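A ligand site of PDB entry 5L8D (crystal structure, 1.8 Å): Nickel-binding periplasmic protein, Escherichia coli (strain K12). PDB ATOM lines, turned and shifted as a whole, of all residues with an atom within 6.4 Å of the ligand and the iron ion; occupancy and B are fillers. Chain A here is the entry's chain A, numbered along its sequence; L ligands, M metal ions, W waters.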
ATOM      1  N   TYR A  22       4.840  -1.765  -7.019  1.00  0.00           N
ATOM      2  CA  TYR A  22       6.292  -1.971  -6.881  1.00  0.00           C
ATOM      3  C   TYR A  22       6.982  -0.765  -7.451  1.00  0.00           C
ATOM      4  O   TYR A  22       6.551   0.346  -7.182  1.00  0.00           O
ATOM      5  CB  TYR A  22       6.672  -3.355  -7.510  1.00  0.00           C
ATOM      6  CG  TYR A  22       5.998  -4.487  -6.877  1.00  0.00           C
ATOM      7  CD1 TYR A  22       4.720  -4.860  -7.300  1.00  0.00           C
ATOM      8  CD2 TYR A  22       6.546  -5.119  -5.839  1.00  0.00           C
ATOM      9  CE1 TYR A  22       4.049  -5.853  -6.708  1.00  0.00           C
ATOM     10  CE2 TYR A  22       5.885  -6.115  -5.171  1.00  0.00           C
ATOM     11  CZ  TYR A  22       4.617  -6.519  -5.656  1.00  0.00           C
ATOM     12  OH  TYR A  22       3.957  -7.539  -5.031  1.00  0.00           O
ATOM     13  N   THR A  23       8.050  -0.916  -8.272  1.00  0.00           N
ATOM     14  CA  THR A  23       8.694   0.206  -8.873  1.00  0.00           C
ATOM     15  C   THR A  23       7.720   1.159  -9.533  1.00  0.00           C
ATOM     16  O   THR A  23       6.748   0.705 -10.163  1.00  0.00           O
ATOM     17  CB  THR A  23       9.817  -0.266  -9.901  1.00  0.00           C
ATOM     18  OG1 THR A  23      10.572   0.887 -10.298  1.00  0.00           O
ATOM     19  CG2 THR A  23       9.254  -0.874 -11.100  1.00  0.00           C
ATOM     20  N   MET A  27      10.497   0.539  -1.187  1.00  0.00           N
ATOM     21  CA  MET A  27       9.981  -0.207  -0.037  1.00  0.00           C
ATOM     22  C   MET A  27      10.182   0.447   1.308  1.00  0.00           C
ATOM     23  O   MET A  27       9.245   0.492   2.203  1.00  0.00           O
ATOM     24  CB  MET A  27      10.553  -1.646   0.047  1.00  0.00           C
ATOM     25  CG  MET A  27       9.825  -2.650  -0.845  1.00  0.00           C
ATOM     26  SD  MET A  27      10.549  -4.319  -0.764  1.00  0.00           S
ATOM     27  CE  MET A  27      12.167  -3.955  -1.423  1.00  0.00           C
ATOM     28  N   ARG A  97       0.089  -9.536 -10.669  1.00  0.00           N
ATOM     29  CA  ARG A  97       1.317  -8.800 -10.338  1.00  0.00           C
ATOM     30  C   ARG A  97       2.040  -9.312  -9.124  1.00  0.00           C
ATOM     31  O   ARG A  97       3.277  -9.097  -8.997  1.00  0.00           O
ATOM     32  CB  ARG A  97       1.032  -7.306 -10.269  1.00  0.00           C
ATOM     33  CG  ARG A  97       2.246  -6.471 -10.019  1.00  0.00           C
ATOM     34  CD  ARG A  97       3.213  -6.463 -11.204  1.00  0.00           C
ATOM     35  NE  ARG A  97       4.491  -5.762 -10.913  1.00  0.00           N
ATOM     36  CZ  ARG A  97       5.545  -6.310 -10.313  1.00  0.00           C
ATOM     37  NH1 ARG A  97       5.486  -7.515  -9.773  1.00  0.00           N
ATOM     38  NH2 ARG A  97       6.676  -5.608 -10.161  1.00  0.00           N
ATOM     39  N   TRP A 100       4.902 -13.677  -7.557  1.00  0.00           N
ATOM     40  CA  TRP A 100       6.128 -14.037  -6.923  1.00  0.00           C
ATOM     41  C   TRP A 100       5.897 -14.367  -5.479  1.00  0.00           C
ATOM     42  O   TRP A 100       6.645 -15.134  -4.914  1.00  0.00           O
ATOM     43  CB  TRP A 100       7.121 -12.877  -7.092  1.00  0.00           C
ATOM     44  CG  TRP A 100       6.703 -11.653  -6.318  1.00  0.00           C
ATOM     45  CD1 TRP A 100       5.946 -10.615  -6.750  1.00  0.00           C
ATOM     46  CD2 TRP A 100       6.992 -11.394  -4.955  1.00  0.00           C
ATOM     47  NE1 TRP A 100       5.738  -9.737  -5.709  1.00  0.00           N
ATOM     48  CE2 TRP A 100       6.399 -10.161  -4.621  1.00  0.00           C
ATOM     49  CE3 TRP A 100       7.749 -12.044  -4.013  1.00  0.00           C
ATOM     50  CZ2 TRP A 100       6.477  -9.613  -3.352  1.00  0.00           C
ATOM     51  CZ3 TRP A 100       7.848 -11.499  -2.769  1.00  0.00           C
ATOM     52  CH2 TRP A 100       7.187 -10.293  -2.437  1.00  0.00           C
ATOM     53  N   LEU A 135       5.428  -8.099   5.440  1.00  0.00           N
ATOM     54  CA  LEU A 135       6.300  -7.528   4.458  1.00  0.00           C
ATOM     55  C   LEU A 135       5.945  -6.023   4.182  1.00  0.00           C
ATOM     56  O   LEU A 135       4.790  -5.653   4.376  1.00  0.00           O
ATOM     57  CB  LEU A 135       6.230  -8.279   3.144  1.00  0.00           C
ATOM     58  CG  LEU A 135       6.740  -9.743   3.208  1.00  0.00           C
ATOM     59  CD1 LEU A 135       6.594 -10.408   1.846  1.00  0.00           C
ATOM     60  CD2 LEU A 135       8.147  -9.778   3.712  1.00  0.00           C
ATOM     61  N   PRO A 136       6.919  -5.207   3.679  1.00  0.00           N
ATOM     62  CA  PRO A 136       6.704  -3.811   3.353  1.00  0.00           C
ATOM     63  C   PRO A 136       5.468  -3.704   2.414  1.00  0.00           C
ATOM     64  O   PRO A 136       4.748  -2.684   2.474  1.00  0.00           O
ATOM     65  CB  PRO A 136       7.982  -3.446   2.592  1.00  0.00           C
ATOM     66  CG  PRO A 136       8.999  -4.217   3.342  1.00  0.00           C
ATOM     67  CD  PRO A 136       8.360  -5.559   3.519  1.00  0.00           C
ATOM     68  N   ARG A 137       5.357  -4.640   1.451  1.00  0.00           N
ATOM     69  CA  ARG A 137       4.296  -4.663   0.419  1.00  0.00           C
ATOM     70  C   ARG A 137       4.054  -6.109   0.037  1.00  0.00           C
ATOM     71  O   ARG A 137       4.979  -6.894   0.057  1.00  0.00           O
ATOM     72  CB  ARG A 137       4.655  -3.798  -0.779  1.00  0.00           C
ATOM     73  CG  ARG A 137       5.939  -4.203  -1.492  1.00  0.00           C
ATOM     74  CD  ARG A 137       6.481  -3.078  -2.333  1.00  0.00           C
ATOM     75  NE  ARG A 137       7.635  -3.506  -3.138  1.00  0.00           N
ATOM     76  CZ  ARG A 137       8.375  -2.686  -3.859  1.00  0.00           C
ATOM     77  NH1 ARG A 137       8.206  -1.384  -3.832  1.00  0.00           N
ATOM     78  NH2 ARG A 137       9.321  -3.162  -4.626  1.00  0.00           N
ATOM     79  N   PRO A 138       2.866  -6.448  -0.429  1.00  0.00           N
ATOM     80  CA  PRO A 138       1.787  -5.488  -0.712  1.00  0.00           C
ATOM     81  C   PRO A 138       0.702  -5.419   0.360  1.00  0.00           C
ATOM     82  O   PRO A 138      -0.160  -4.604   0.215  1.00  0.00           O
ATOM     83  CB  PRO A 138       1.142  -6.087  -1.946  1.00  0.00           C
ATOM     84  CG  PRO A 138       1.280  -7.561  -1.702  1.00  0.00           C
ATOM     85  CD  PRO A 138       2.635  -7.740  -1.068  1.00  0.00           C
ATOM     86  N   GLU A 247      22.146 -10.477   3.165  1.00  0.00           N
ATOM     87  CA  GLU A 247      21.722 -11.255   1.995  1.00  0.00           C
ATOM     88  C   GLU A 247      22.940 -11.595   1.163  1.00  0.00           C
ATOM     89  O   GLU A 247      24.041 -11.053   1.399  1.00  0.00           O
ATOM     90  CB  GLU A 247      20.690 -10.450   1.181  1.00  0.00           C
ATOM     91  CG  GLU A 247      21.274  -9.214   0.518  1.00  0.00           C
ATOM     92  CD  GLU A 247      20.258  -8.075   0.299  1.00  0.00           C
ATOM     93  OE1 GLU A 247      19.184  -7.998   0.956  1.00  0.00           O
ATOM     94  OE2 GLU A 247      20.521  -7.246  -0.596  1.00  0.00           O
ATOM     95  N   GLN A 385      17.048 -10.848 -17.376  1.00  0.00           N
ATOM     96  CA  GLN A 385      16.748 -11.758 -16.268  1.00  0.00           C
ATOM     97  C   GLN A 385      15.413 -12.457 -16.492  1.00  0.00           C
ATOM     98  O   GLN A 385      15.282 -13.659 -16.214  1.00  0.00           O
ATOM     99  CB  GLN A 385      16.683 -10.974 -14.961  1.00  0.00           C
ATOM    100  CG  GLN A 385      18.022 -10.542 -14.453  1.00  0.00           C
ATOM    101  CD  GLN A 385      17.963  -9.880 -13.049  1.00  0.00           C
ATOM    102  OE1 GLN A 385      16.920  -9.413 -12.626  1.00  0.00           O
ATOM    103  NE2 GLN A 385      19.065  -9.920 -12.334  1.00  0.00           N
ATOM    104  N   HIS A 395      23.114 -11.151  -9.388  1.00  0.00           N
ATOM    105  CA  HIS A 395      21.808 -11.363  -8.802  1.00  0.00           C
ATOM    106  C   HIS A 395      22.048 -11.279  -7.310  1.00  0.00           C
ATOM    107  O   HIS A 395      23.228 -11.264  -6.797  1.00  0.00           O
ATOM    108  CB  HIS A 395      21.277 -12.712  -9.284  1.00  0.00           C
ATOM    109  CG  HIS A 395      19.804 -12.960  -9.002  1.00  0.00           C
ATOM    110  ND1 HIS A 395      18.890 -11.946  -8.792  1.00  0.00           N
ATOM    111  CD2 HIS A 395      19.138 -14.117  -8.766  1.00  0.00           C
ATOM    112  CE1 HIS A 395      17.705 -12.467  -8.528  1.00  0.00           C
ATOM    113  NE2 HIS A 395      17.818 -13.789  -8.531  1.00  0.00           N
ATOM    114  N   ARG A 396      20.962 -11.278  -6.558  1.00  0.00           N
ATOM    115  CA  ARG A 396      21.030 -11.222  -5.131  1.00  0.00           C
ATOM    116  C   ARG A 396      19.820 -11.845  -4.495  1.00  0.00           C
ATOM    117  O   ARG A 396      18.712 -11.909  -5.063  1.00  0.00           O
ATOM    118  CB  ARG A 396      21.262  -9.784  -4.606  1.00  0.00           C
ATOM    119  CG  ARG A 396      20.198  -8.788  -4.945  1.00  0.00           C
ATOM    120  CD  ARG A 396      20.675  -7.324  -4.816  1.00  0.00           C
ATOM    121  NE  ARG A 396      21.231  -6.993  -3.494  1.00  0.00           N
ATOM    122  CZ  ARG A 396      22.396  -6.374  -3.306  1.00  0.00           C
ATOM    123  NH1 ARG A 396      23.143  -5.928  -4.304  1.00  0.00           N
ATOM    124  NH2 ARG A 396      22.787  -6.113  -2.080  1.00  0.00           N
ATOM    125  N   THR A 397      20.007 -12.343  -3.283  1.00  0.00           N
ATOM    126  CA  THR A 397      18.878 -12.776  -2.482  1.00  0.00           C
ATOM    127  C   THR A 397      18.231 -11.571  -1.779  1.00  0.00           C
ATOM    128  O   THR A 397      18.595 -10.415  -2.022  1.00  0.00           O
ATOM    129  CB  THR A 397      19.167 -13.910  -1.476  1.00  0.00           C
ATOM    130  OG1 THR A 397      19.972 -13.448  -0.383  1.00  0.00           O
ATOM    131  CG2 THR A 397      19.809 -15.118  -2.191  1.00  0.00           C
ATOM    132  N   TRP A 398      17.193 -11.829  -0.991  1.00  0.00           N
ATOM    133  CA  TRP A 398      16.300 -10.712  -0.598  1.00  0.00           C
ATOM    134  C   TRP A 398      16.386 -10.325   0.849  1.00  0.00           C
ATOM    135  O   TRP A 398      15.752  -9.407   1.251  1.00  0.00           O
ATOM    136  CB  TRP A 398      14.860 -11.094  -0.998  1.00  0.00           C
ATOM    137  CG  TRP A 398      14.643 -11.201  -2.495  1.00  0.00           C
ATOM    138  CD1 TRP A 398      15.423 -10.697  -3.458  1.00  0.00           C
ATOM    139  CD2 TRP A 398      13.495 -11.792  -3.178  1.00  0.00           C
ATOM    140  NE1 TRP A 398      14.877 -10.956  -4.698  1.00  0.00           N
ATOM    141  CE2 TRP A 398      13.705 -11.639  -4.548  1.00  0.00           C
ATOM    142  CE3 TRP A 398      12.385 -12.492  -2.748  1.00  0.00           C
ATOM    143  CZ2 TRP A 398      12.816 -12.117  -5.500  1.00  0.00           C
ATOM    144  CZ3 TRP A 398      11.472 -12.993  -3.741  1.00  0.00           C
ATOM    145  CH2 TRP A 398      11.711 -12.805  -5.068  1.00  0.00           C
ATOM    146  N   TYR A 402      12.283 -12.697   3.676  1.00  0.00           N
ATOM    147  CA  TYR A 402      12.192 -13.412   2.412  1.00  0.00           C
ATOM    148  C   TYR A 402      13.041 -14.685   2.277  1.00  0.00           C
ATOM    149  O   TYR A 402      12.624 -15.666   1.575  1.00  0.00           O
ATOM    150  CB  TYR A 402      12.575 -12.494   1.214  1.00  0.00           C
ATOM    151  CG  TYR A 402      11.861 -11.195   1.182  1.00  0.00           C
ATOM    152  CD1 TYR A 402      10.637 -11.074   0.499  1.00  0.00           C
ATOM    153  CD2 TYR A 402      12.382 -10.026   1.815  1.00  0.00           C
ATOM    154  CE1 TYR A 402       9.963  -9.824   0.475  1.00  0.00           C
ATOM    155  CE2 TYR A 402      11.692  -8.805   1.773  1.00  0.00           C
ATOM    156  CZ  TYR A 402      10.512  -8.709   1.090  1.00  0.00           C
ATOM    157  OH  TYR A 402       9.831  -7.494   1.062  1.00  0.00           O
ATOM    158  N   HIS A 416      11.393 -14.638 -13.741  1.00  0.00           N
ATOM    159  CA  HIS A 416      12.406 -14.197 -12.806  1.00  0.00           C
ATOM    160  C   HIS A 416      13.711 -14.901 -13.148  1.00  0.00           C
ATOM    161  O   HIS A 416      13.737 -16.002 -13.705  1.00  0.00           O
ATOM    162  CB  HIS A 416      11.994 -14.536 -11.385  1.00  0.00           C
ATOM    163  CG  HIS A 416      10.903 -13.673 -10.831  1.00  0.00           C
ATOM    164  ND1 HIS A 416      10.760 -13.456  -9.476  1.00  0.00           N
ATOM    165  CD2 HIS A 416       9.933 -12.942 -11.434  1.00  0.00           C
ATOM    166  CE1 HIS A 416       9.744 -12.633  -9.268  1.00  0.00           C
ATOM    167  NE2 HIS A 416       9.231 -12.305 -10.445  1.00  0.00           N
ATOM    168  N   THR A 490      14.937  -4.633   3.881  1.00  0.00           N
ATOM    169  CA  THR A 490      14.599  -3.480   3.029  1.00  0.00           C
ATOM    170  C   THR A 490      14.021  -2.267   3.754  1.00  0.00           C
ATOM    171  O   THR A 490      13.714  -1.252   3.152  1.00  0.00           O
ATOM    172  CB  THR A 490      13.596  -3.902   1.942  1.00  0.00           C
ATOM    173  OG1 THR A 490      12.444  -4.505   2.513  1.00  0.00           O
ATOM    174  CG2 THR A 490      14.205  -4.981   1.028  1.00  0.00           C
HETATM  175  O1  LIG L   1      12.797  -6.085  -3.929  1.00  0.00           O
HETATM  176  C1  LIG L   1      13.190  -6.901  -3.014  1.00  0.00           C
HETATM  177  O2  LIG L   1      14.147  -6.768  -2.214  1.00  0.00           O
HETATM  178  C2  LIG L   1      12.485  -8.174  -2.862  1.00  0.00           C
HETATM  179  N1  LIG L   1      11.221  -8.115  -3.624  1.00  0.00           N
HETATM  180  C3  LIG L   1      10.154  -7.669  -2.728  1.00  0.00           C
HETATM  181  C4  LIG L   1       9.304  -6.591  -3.373  1.00  0.00           C
HETATM  182  O3  LIG L   1       9.651  -5.951  -4.424  1.00  0.00           O
HETATM  183  O4  LIG L   1       8.266  -6.381  -2.717  1.00  0.00           O
HETATM  184  C5  LIG L   1      10.877  -9.458  -4.165  1.00  0.00           C
HETATM  185  C6  LIG L   1       9.806  -9.432  -5.228  1.00  0.00           C
HETATM  186  N2  LIG L   1      10.289  -8.444  -6.201  1.00  0.00           N
HETATM  187  C7  LIG L   1      11.081  -9.038  -7.275  1.00  0.00           C
HETATM  188  C8  LIG L   1      12.594  -8.776  -7.083  1.00  0.00           C
HETATM  189  O5  LIG L   1      12.977  -7.870  -6.324  1.00  0.00           O
HETATM  190  O6  LIG L   1      13.441  -9.488  -7.668  1.00  0.00           O
HETATM  191  C9  LIG L   1       9.139  -7.730  -6.818  1.00  0.00           C
HETATM  192  C10 LIG L   1       9.600  -6.526  -7.582  1.00  0.00           C
HETATM  193  O7  LIG L   1      10.667  -5.947  -7.186  1.00  0.00           O
HETATM  194  O8  LIG L   1       8.889  -6.148  -8.531  1.00  0.00           O
HETATM  195 FE    FE M   1      11.484  -6.633  -5.359  1.00  0.00          FE
HETATM  196  O   HOH W   1      15.426  -4.354  -2.610  1.00  0.00           O
HETATM  197  O   HOH W   2       7.673  -7.222  -0.299  1.00  0.00           O
HETATM  198  O   HOH W   3       9.541  -3.543  -9.248  1.00  0.00           O
HETATM  199  O   HOH W   4      11.979  -4.675  -5.931  1.00  0.00           O
HETATM  200  O   HOH W   5      12.133  -3.111  -8.258  1.00  0.00           O
HETATM  201  O   HOH W   6      14.042 -12.075  -8.772  1.00  0.00           O
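The side-chain sulfur (SD) of Met 27 sits at hydrogen-bond distance from the side-chain hydroxyl (OG1) of Thr 490, at 3.8 Å. SD of Met 27 lies within hydrogen-bond range of OH of Tyr 402 (3.7 Å). OH of Tyr 22 is in hydrogen-bond range of NE1 of Trp 100, 2.9 Å away.
Water W2 lies within hydrogen-bond range of OH of Tyr 402 (2.6 Å), O4 of the ligand (2.6 Å) and O of Arg 137 (2.7 Å). Water W3 bridges an oxygen (O8) of the ligand (2.8 Å) and the backbone NH of Thr 23 (3.2 Å).
No residue comes within 4 Å of the iron ion. The nearest printed residue that does not touch the iron ion is Arg 137 (4.2 Å).
An oxygen (O4) of the ligand is in salt-bridge range of the guanidinium group (NE) of Arg 137 (3.0 Å). An oxygen (O8) of the ligand lies within salt-bridge range of the guanidinium group (NH2) of Arg 97 (2.8 Å).
The iron ion is bound by O1 of the ligand (2.0 Å), water W4 (2.1 Å), O7 of the ligand (2.1 Å), O5 of the ligand (2.2 Å), O3 of the ligand (2.2 Å), N1 of the ligand (2.3 Å) and N2 of the ligand (2.3 Å). The iron ion has seven donor atoms within binding distance.
SD of Met 27 sits close to O4 of the ligand, 3.6 Å away. Tyr 22 touches the ligand (CE2 to O4, 3.4 Å). Trp 100 touches the ligand (CD2 to C6, 3.4 Å). Trp 398 touches the ligand. Tyr 402 touches the ligand (OH to C3, 3.8 Å). Thr 490 touches the ligand. Eight residues have an atom within 4 Å of the ligand: Tyr 22, Met 27, Arg 97, Trp 100, Arg 137, Trp 398, Tyr 402 and Thr 490.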
